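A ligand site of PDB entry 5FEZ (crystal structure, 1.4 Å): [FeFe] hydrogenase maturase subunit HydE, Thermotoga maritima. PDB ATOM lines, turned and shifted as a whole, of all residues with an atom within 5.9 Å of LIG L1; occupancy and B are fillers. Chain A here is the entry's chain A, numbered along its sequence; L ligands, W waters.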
ATOM      1  N   TYR A  79      15.187 -11.512  22.459  1.00  0.00           N
ATOM      2  CA  TYR A  79      14.425 -11.966  21.280  1.00  0.00           C
ATOM      3  C   TYR A  79      13.369 -10.993  20.779  1.00  0.00           C
ATOM      4  O   TYR A  79      12.877 -11.156  19.653  1.00  0.00           O
ATOM      5  CB  TYR A  79      13.792 -13.334  21.530  1.00  0.00           C
ATOM      6  CG  TYR A  79      13.121 -13.498  22.868  1.00  0.00           C
ATOM      7  CD1 TYR A  79      11.832 -12.990  23.065  1.00  0.00           C
ATOM      8  CD2 TYR A  79      13.746 -14.073  23.964  1.00  0.00           C
ATOM      9  CE1 TYR A  79      11.218 -13.084  24.288  1.00  0.00           C
ATOM     10  CE2 TYR A  79      13.122 -14.132  25.179  1.00  0.00           C
ATOM     11  CZ  TYR A  79      11.838 -13.646  25.336  1.00  0.00           C
ATOM     12  OH  TYR A  79      11.269 -13.757  26.585  1.00  0.00           O
ATOM     13  N   CYS A  80      13.000 -10.042  21.627  1.00  0.00           N
ATOM     14  CA  CYS A  80      11.748  -9.328  21.447  1.00  0.00           C
ATOM     15  C   CYS A  80      11.841  -7.968  20.802  1.00  0.00           C
ATOM     16  O   CYS A  80      12.609  -7.124  21.279  1.00  0.00           O
ATOM     17  CB  CYS A  80      11.072  -9.159  22.793  1.00  0.00           C
ATOM     18  SG  CYS A  80       9.425  -8.384  22.759  1.00  0.00           S
ATOM     19  N   GLY A  81      11.056  -7.692  19.761  1.00  0.00           N
ATOM     20  CA  GLY A  81      11.057  -6.408  19.157  1.00  0.00           C
ATOM     21  C   GLY A  81      10.595  -5.230  19.992  1.00  0.00           C
ATOM     22  O   GLY A  81      10.831  -4.079  19.595  1.00  0.00           O
ATOM     23  N   GLN A 117      -3.091  -7.684  26.381  1.00  0.00           N
ATOM     24  CA  GLN A 117      -1.674  -7.940  26.358  1.00  0.00           C
ATOM     25  C   GLN A 117      -0.935  -6.649  26.188  1.00  0.00           C
ATOM     26  O   GLN A 117      -1.351  -5.766  25.443  1.00  0.00           O
ATOM     27  CB  GLN A 117      -1.272  -8.975  25.270  1.00  0.00           C
ATOM     28  CG  GLN A 117       0.183  -9.440  25.407  1.00  0.00           C
ATOM     29  CD  GLN A 117       0.573 -10.402  24.333  1.00  0.00           C
ATOM     30  OE1 GLN A 117       0.933  -9.977  23.239  1.00  0.00           O
ATOM     31  NE2 GLN A 117       0.532 -11.652  24.612  1.00  0.00           N
ATOM     32  N   SER A 146      -2.271 -10.662  30.023  1.00  0.00           N
ATOM     33  CA  SER A 146      -0.908 -11.091  29.590  1.00  0.00           C
ATOM     34  C   SER A 146      -0.010  -9.855  29.684  1.00  0.00           C
ATOM     35  O   SER A 146       0.312  -9.237  28.707  1.00  0.00           O
ATOM     36  CB  SER A 146      -0.948 -11.637  28.177  1.00  0.00           C
ATOM     37  OG  SER A 146       0.283 -12.204  27.794  1.00  0.00           O
ATOM     38  N   ARG A 169       4.005 -17.056  29.405  1.00  0.00           N
ATOM     39  CA  ARG A 169       4.807 -18.130  28.875  1.00  0.00           C
ATOM     40  C   ARG A 169       6.013 -18.322  29.720  1.00  0.00           C
ATOM     41  O   ARG A 169       6.673 -17.353  30.084  1.00  0.00           O
ATOM     42  CB  ARG A 169       5.195 -17.860  27.461  1.00  0.00           C
ATOM     43  CG  ARG A 169       4.017 -17.994  26.480  1.00  0.00           C
ATOM     44  CD  ARG A 169       4.616 -17.860  25.128  1.00  0.00           C
ATOM     45  NE  ARG A 169       3.601 -17.911  24.114  1.00  0.00           N
ATOM     46  CZ  ARG A 169       3.889 -17.994  22.831  1.00  0.00           C
ATOM     47  NH1 ARG A 169       5.166 -18.004  22.379  1.00  0.00           N
ATOM     48  NH2 ARG A 169       2.931 -18.139  21.972  1.00  0.00           N
ATOM     49  N   GLU A 171       8.768 -19.464  28.510  1.00  0.00           N
ATOM     50  CA  GLU A 171       9.758 -19.143  27.479  1.00  0.00           C
ATOM     51  C   GLU A 171      10.772 -20.244  27.177  1.00  0.00           C
ATOM     52  O   GLU A 171      10.897 -20.702  26.078  1.00  0.00           O
ATOM     53  CB  GLU A 171      10.440 -17.788  27.747  1.00  0.00           C
ATOM     54  CG  GLU A 171       9.499 -16.625  28.091  1.00  0.00           C
ATOM     55  CD  GLU A 171       8.553 -16.255  26.988  1.00  0.00           C
ATOM     56  OE1 GLU A 171       8.427 -16.902  25.965  1.00  0.00           O
ATOM     57  OE2 GLU A 171       7.855 -15.253  27.195  1.00  0.00           O
ATOM     58  N   ARG A 190      10.063 -16.305  37.005  1.00  0.00           N
ATOM     59  CA  ARG A 190       8.957 -16.658  36.096  1.00  0.00           C
ATOM     60  C   ARG A 190       8.074 -17.727  36.669  1.00  0.00           C
ATOM     61  O   ARG A 190       6.841 -17.648  36.673  1.00  0.00           O
ATOM     62  CB  ARG A 190       9.562 -17.098  34.753  1.00  0.00           C
ATOM     63  CG  ARG A 190       8.596 -17.085  33.543  1.00  0.00           C
ATOM     64  CD  ARG A 190       8.383 -15.658  33.117  1.00  0.00           C
ATOM     65  NE  ARG A 190       7.688 -15.561  31.810  1.00  0.00           N
ATOM     66  CZ  ARG A 190       7.311 -14.395  31.267  1.00  0.00           C
ATOM     67  NH1 ARG A 190       7.608 -13.265  31.875  1.00  0.00           N
ATOM     68  NH2 ARG A 190       6.638 -14.422  30.152  1.00  0.00           N
ATOM     69  N   SER A 208       6.249 -21.892  25.533  1.00  0.00           N
ATOM     70  CA  SER A 208       7.656 -21.698  25.224  1.00  0.00           C
ATOM     71  C   SER A 208       7.831 -21.416  23.782  1.00  0.00           C
ATOM     72  O   SER A 208       6.953 -21.660  22.955  1.00  0.00           O
ATOM     73  CB  SER A 208       8.492 -22.848  25.689  1.00  0.00           C
ATOM     74  OG  SER A 208       7.958 -24.061  25.227  1.00  0.00           O
ATOM     75  N   MET A 209       9.037 -20.878  23.453  1.00  0.00           N
ATOM     76  CA  MET A 209       9.439 -20.743  22.063  1.00  0.00           C
ATOM     77  C   MET A 209      10.330 -21.948  21.674  1.00  0.00           C
ATOM     78  O   MET A 209      10.986 -22.554  22.533  1.00  0.00           O
ATOM     79  CB  MET A 209      10.211 -19.467  21.832  1.00  0.00           C
ATOM     80  CG  MET A 209       9.310 -18.203  21.844  1.00  0.00           C
ATOM     81  SD  MET A 209      10.259 -16.649  21.786  1.00  0.00           S
ATOM     82  CE  MET A 209      10.811 -16.580  23.441  1.00  0.00           C
ATOM     83  N   GLY A 238       5.171 -21.373  20.076  1.00  0.00           N
ATOM     84  CA  GLY A 238       5.443 -20.943  18.736  1.00  0.00           C
ATOM     85  C   GLY A 238       6.948 -21.008  18.456  1.00  0.00           C
ATOM     86  O   GLY A 238       7.760 -21.137  19.382  1.00  0.00           O
ATOM     87  N   PRO A 239       7.279 -20.826  17.190  1.00  0.00           N
ATOM     88  CA  PRO A 239       8.693 -20.768  16.810  1.00  0.00           C
ATOM     89  C   PRO A 239       9.286 -19.446  17.143  1.00  0.00           C
ATOM     90  O   PRO A 239       8.630 -18.413  17.096  1.00  0.00           O
ATOM     91  CB  PRO A 239       8.657 -20.926  15.287  1.00  0.00           C
ATOM     92  CG  PRO A 239       7.361 -20.243  14.920  1.00  0.00           C
ATOM     93  CD  PRO A 239       6.435 -20.644  16.014  1.00  0.00           C
ATOM     94  N   PHE A 240      10.591 -19.430  17.475  1.00  0.00           N
ATOM     95  CA  PHE A 240      11.345 -18.190  17.554  1.00  0.00           C
ATOM     96  C   PHE A 240      11.507 -17.604  16.165  1.00  0.00           C
ATOM     97  O   PHE A 240      11.868 -18.332  15.224  1.00  0.00           O
ATOM     98  CB  PHE A 240      12.740 -18.468  18.117  1.00  0.00           C
ATOM     99  CG  PHE A 240      13.686 -17.358  17.921  1.00  0.00           C
ATOM    100  CD1 PHE A 240      13.533 -16.126  18.516  1.00  0.00           C
ATOM    101  CD2 PHE A 240      14.806 -17.588  17.121  1.00  0.00           C
ATOM    102  CE1 PHE A 240      14.428 -15.073  18.228  1.00  0.00           C
ATOM    103  CE2 PHE A 240      15.728 -16.570  16.891  1.00  0.00           C
ATOM    104  CZ  PHE A 240      15.523 -15.323  17.432  1.00  0.00           C
ATOM    105  N   ILE A 241      11.216 -16.302  16.017  1.00  0.00           N
ATOM    106  CA  ILE A 241      11.327 -15.633  14.752  1.00  0.00           C
ATOM    107  C   ILE A 241      12.258 -14.425  14.971  1.00  0.00           C
ATOM    108  O   ILE A 241      11.901 -13.468  15.683  1.00  0.00           O
ATOM    109  CB  ILE A 241       9.970 -15.212  14.174  1.00  0.00           C
ATOM    110  CG1 ILE A 241       9.073 -16.423  13.955  1.00  0.00           C
ATOM    111  CG2 ILE A 241      10.161 -14.385  12.905  1.00  0.00           C
ATOM    112  CD1 ILE A 241       7.622 -16.047  13.598  1.00  0.00           C
ATOM    113  N   PRO A 242      13.456 -14.391  14.368  1.00  0.00           N
ATOM    114  CA  PRO A 242      14.386 -13.287  14.653  1.00  0.00           C
ATOM    115  C   PRO A 242      13.847 -11.952  14.199  1.00  0.00           C
ATOM    116  O   PRO A 242      13.264 -11.785  13.124  1.00  0.00           O
ATOM    117  CB  PRO A 242      15.651 -13.680  13.866  1.00  0.00           C
ATOM    118  CG  PRO A 242      15.140 -14.533  12.777  1.00  0.00           C
ATOM    119  CD  PRO A 242      13.938 -15.268  13.276  1.00  0.00           C
ATOM    120  N   HIS A 243      14.090 -10.962  15.068  1.00  0.00           N
ATOM    121  CA  HIS A 243      13.634  -9.615  14.797  1.00  0.00           C
ATOM    122  C   HIS A 243      14.904  -8.731  14.508  1.00  0.00           C
ATOM    123  O   HIS A 243      15.889  -8.767  15.238  1.00  0.00           O
ATOM    124  CB  HIS A 243      12.880  -9.062  16.002  1.00  0.00           C
ATOM    125  CG  HIS A 243      12.220  -7.741  15.789  1.00  0.00           C
ATOM    126  ND1 HIS A 243      12.909  -6.575  15.529  1.00  0.00           N
ATOM    127  CD2 HIS A 243      10.912  -7.416  15.799  1.00  0.00           C
ATOM    128  CE1 HIS A 243      12.045  -5.597  15.369  1.00  0.00           C
ATOM    129  NE2 HIS A 243      10.830  -6.093  15.534  1.00  0.00           N
ATOM    130  N   ALA A 280       2.358 -16.797  15.471  1.00  0.00           N
ATOM    131  CA  ALA A 280       3.724 -17.082  15.023  1.00  0.00           C
ATOM    132  C   ALA A 280       3.790 -18.292  14.099  1.00  0.00           C
ATOM    133  O   ALA A 280       4.493 -18.272  13.136  1.00  0.00           O
ATOM    134  CB  ALA A 280       4.664 -17.211  16.195  1.00  0.00           C
ATOM    135  N   LEU A 315       6.466  -8.142  17.885  1.00  0.00           N
ATOM    136  CA  LEU A 315       7.403  -8.866  18.695  1.00  0.00           C
ATOM    137  C   LEU A 315       8.429  -9.507  17.770  1.00  0.00           C
ATOM    138  O   LEU A 315       9.575  -9.619  18.090  1.00  0.00           O
ATOM    139  CB  LEU A 315       6.674  -9.974  19.471  1.00  0.00           C
ATOM    140  CG  LEU A 315       5.461  -9.507  20.266  1.00  0.00           C
ATOM    141  CD1 LEU A 315       4.851 -10.657  21.027  1.00  0.00           C
ATOM    142  CD2 LEU A 315       5.792  -8.399  21.101  1.00  0.00           C
ATOM    143  N   TYR A 316       7.942  -9.932  16.621  1.00  0.00           N
ATOM    144  CA  TYR A 316       8.716 -10.544  15.556  1.00  0.00           C
ATOM    145  C   TYR A 316       8.178  -9.947  14.256  1.00  0.00           C
ATOM    146  O   TYR A 316       7.081  -9.496  14.213  1.00  0.00           O
ATOM    147  CB  TYR A 316       8.613 -12.080  15.553  1.00  0.00           C
ATOM    148  CG  TYR A 316       7.181 -12.601  15.625  1.00  0.00           C
ATOM    149  CD1 TYR A 316       6.400 -12.689  14.483  1.00  0.00           C
ATOM    150  CD2 TYR A 316       6.602 -12.944  16.827  1.00  0.00           C
ATOM    151  CE1 TYR A 316       5.113 -13.129  14.535  1.00  0.00           C
ATOM    152  CE2 TYR A 316       5.293 -13.366  16.883  1.00  0.00           C
ATOM    153  CZ  TYR A 316       4.580 -13.462  15.755  1.00  0.00           C
ATOM    154  OH  TYR A 316       3.302 -13.854  15.795  1.00  0.00           O
ATOM    155  N   PRO A 317       8.905  -9.917  13.216  1.00  0.00           N
ATOM    156  CA  PRO A 317       8.429  -9.354  11.961  1.00  0.00           C
ATOM    157  C   PRO A 317       7.528 -10.256  11.219  1.00  0.00           C
ATOM    158  O   PRO A 317       7.523 -11.481  11.358  1.00  0.00           O
ATOM    159  CB  PRO A 317       9.689  -9.240  11.101  1.00  0.00           C
ATOM    160  CG  PRO A 317      10.686 -10.233  11.685  1.00  0.00           C
ATOM    161  CD  PRO A 317      10.310 -10.341  13.160  1.00  0.00           C
HETATM  162  N1  LIG L   1       9.707 -14.698  18.000  1.00  0.00           N
HETATM  163  C1  LIG L   1       8.649 -15.445  18.362  1.00  0.00           C
HETATM  164  N2  LIG L   1       7.943 -15.272  19.493  1.00  0.00           N
HETATM  165  C2  LIG L   1       8.267 -14.263  20.258  1.00  0.00           C
HETATM  166  N3  LIG L   1       7.749 -13.809  21.374  1.00  0.00           N
HETATM  167  C3  LIG L   1       8.454 -12.711  21.706  1.00  0.00           C
HETATM  168  N4  LIG L   1       9.377 -12.445  20.830  1.00  0.00           N
HETATM  169  C4  LIG L   1       9.299 -13.396  19.869  1.00  0.00           C
HETATM  170  C5  LIG L   1      10.033 -13.661  18.692  1.00  0.00           C
HETATM  171  N5  LIG L   1      11.064 -12.879  18.272  1.00  0.00           N
HETATM  172  C6  LIG L   1       6.764 -14.534  22.166  1.00  0.00           C
HETATM  173  C7  LIG L   1       7.231 -14.821  23.591  1.00  0.00           C
HETATM  174  C8  LIG L   1       6.205 -14.094  24.417  1.00  0.00           C
HETATM  175  C9  LIG L   1       4.982 -14.131  23.534  1.00  0.00           C
HETATM  176  C10 LIG L   1       4.070 -12.970  23.770  1.00  0.00           C
HETATM  177  O1  LIG L   1       5.566 -13.804  22.263  1.00  0.00           O
HETATM  178  O2  LIG L   1       7.184 -16.245  23.777  1.00  0.00           O
HETATM  179  O3  LIG L   1       5.871 -14.721  25.674  1.00  0.00           O
HETATM  180  N1  LG2 L   2       5.395  -8.785  28.251  1.00  0.00           N
HETATM  181  C1  LG2 L   2       4.517  -9.928  28.586  1.00  0.00           C
HETATM  182  C2  LG2 L   2       5.354 -11.197  28.725  1.00  0.00           C
HETATM  183  O1  LG2 L   2       4.917 -12.184  29.275  1.00  0.00           O
HETATM  184  C3  LG2 L   2       3.467 -10.054  27.500  1.00  0.00           C
HETATM  185  C4  LG2 L   2       3.930 -10.865  26.291  1.00  0.00           C
HETATM  186  S1  LG2 L   2       5.342 -10.154  25.435  1.00  0.00           S
HETATM  187  C5  LG2 L   2       4.385  -8.740  24.755  1.00  0.00           C
HETATM  188  O2  LG2 L   2       6.532 -11.039  28.241  1.00  0.00           O
HETATM  189  C1  LG3 L   3      -0.008 -15.675  21.993  1.00  0.00           C
HETATM  190  C2  LG3 L   3       2.292 -14.517  21.133  1.00  0.00           C
HETATM  191  O1  LG3 L   3       0.197 -17.947  22.331  1.00  0.00           O
HETATM  192  C3  LG3 L   3      -0.327 -16.956  22.717  1.00  0.00           C
HETATM  193  O2  LG3 L   3      -1.010 -16.956  23.763  1.00  0.00           O
HETATM  194  N1  LG3 L   3       0.357 -15.891  20.599  1.00  0.00           N
HETATM  195  C4  LG3 L   3      -1.199 -14.683  22.071  1.00  0.00           C
HETATM  196 SE1  LG3 L   3       1.470 -14.812  22.891  1.00  0.00          SE
HETATM  197  C5  LG3 L   3       1.250 -14.773  20.129  1.00  0.00           C
HETATM  198  C6  LG3 L   3       1.844 -15.038  18.748  1.00  0.00           C
HETATM  199  O3  LG3 L   3       2.050 -13.969  18.104  1.00  0.00           O
HETATM  200  O4  LG3 L   3       2.110 -16.083  18.327  1.00  0.00           O
HETATM  201 SE1  LG4 L   4      10.922  -7.246  26.091  1.00  0.00          SE
HETATM  202 FE1  LG4 L   4       9.031  -8.301  24.985  1.00  0.00          FE
HETATM  203 FE2  LG4 L   4      10.259  -9.258  27.214  1.00  0.00          FE
HETATM  204 FE3  LG4 L   4       8.941  -6.863  27.273  1.00  0.00          FE
HETATM  205 SE2  LG4 L   4       7.209  -7.182  25.723  1.00  0.00          SE
HETATM  206 FE4  LG4 L   4       7.225  -9.259  27.035  1.00  0.00          FE
HETATM  207 SE3  LG4 L   4       8.904 -10.549  25.721  1.00  0.00          SE
HETATM  208 SE4  LG4 L   4       8.818  -8.554  28.941  1.00  0.00          SE
HETATM  209  O   HOH W   1       6.421 -17.637  19.407  1.00  0.00           O
HETATM  210  O   HOH W   2       4.124 -14.445  27.775  1.00  0.00           O
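O3 of LIG L1 is in hydrogen-bond range of OE2 of Glu 171. N of Ile 241 is in hydrogen-bond range of N1 of LIG L1. The backbone carbonyl oxygen (O) of Ile 241 sits at hydrogen-bond distance from a nitrogen (N5) of LIG L1. O of Tyr 79 sits at hydrogen-bond distance from N5 of LIG L1, at 2.9 Å. NH1 of Arg 169 sits at hydrogen-bond distance from O2 of LIG L1, at 3.0 Å. The side-chain sulfur (SD) of Met 209 sits close to an oxygen (O2) of LIG L1, 3.7 Å away. The guanidinium group (NH2) of Arg 190 is in salt-bridge range of an oxygen (O1) of LG2 L2, 3.0 Å away. An oxygen (O1) of LG3 L3 lies within salt-bridge range of the guanidinium group (NH2) of Arg 169 (2.8 Å). The side-chain hydroxyl (OH) of Tyr 316 sits at hydrogen-bond distance from an oxygen (O3) of LG3 L3 (2.6 Å). An oxygen (O4) of LG3 L3 lies within hydrogen-bond range of the backbone NH (N) of Ala 280 (3.0 Å). An iron atom (FE1) of LG4 L4 is bound by the side-chain sulfur of Cys 80 (2.3 Å).
N of Met 209 sits at hydrogen-bond distance from O of Glu 171 (3.2 Å). NH2 of Arg 190 is in salt-bridge range of OE2 of Glu 171. The guanidinium group of Arg 190 sits at hydrogen-bond distance from the backbone carbonyl oxygen of Arg 169 (2.7 Å). O of Leu 315 lies within hydrogen-bond range of N of Gly 81, at 2.9 Å. OH of Tyr 316 sits at hydrogen-bond distance from N of Ala 280, 3.1 Å away. The side-chain amide nitrogen (NE2) of Gln 117 sits at hydrogen-bond distance from the side-chain hydroxyl (OG) of Ser 146 (3.2 Å).
CA of Cys 80 touches N4 of LIG L1 (3.96 Å). Gln 117 touches LIG L1. Pro 239 touches LIG L1. C of Phe 240 touches N1 of LIG L1, at 3.9 Å. Leu 315 touches LIG L1. Tyr 316 touches LIG L1 (CD2 to C1, 3.6 Å). Hydrophobic or aromatic side chains that line LIG L1: Tyr 79, Met 209, Ile 241, Leu 315 and Tyr 316. The nearest printed residue that does not touch LIG L1 is Arg 190 (4.6 Å).
Water W2 lies within hydrogen-bond range of O3 of LIG L1, O1 of LG2 L2, N of Arg 169 and NH2 of Arg 190. Water W1 lies within hydrogen-bond range of N2 of LIG L1, NH1 of Arg 169 and O of Pro 239.
An iron atom (FE4) of LG4 L4 is bound by a nitrogen (N1) of LG2 L2 (2.2 Å).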
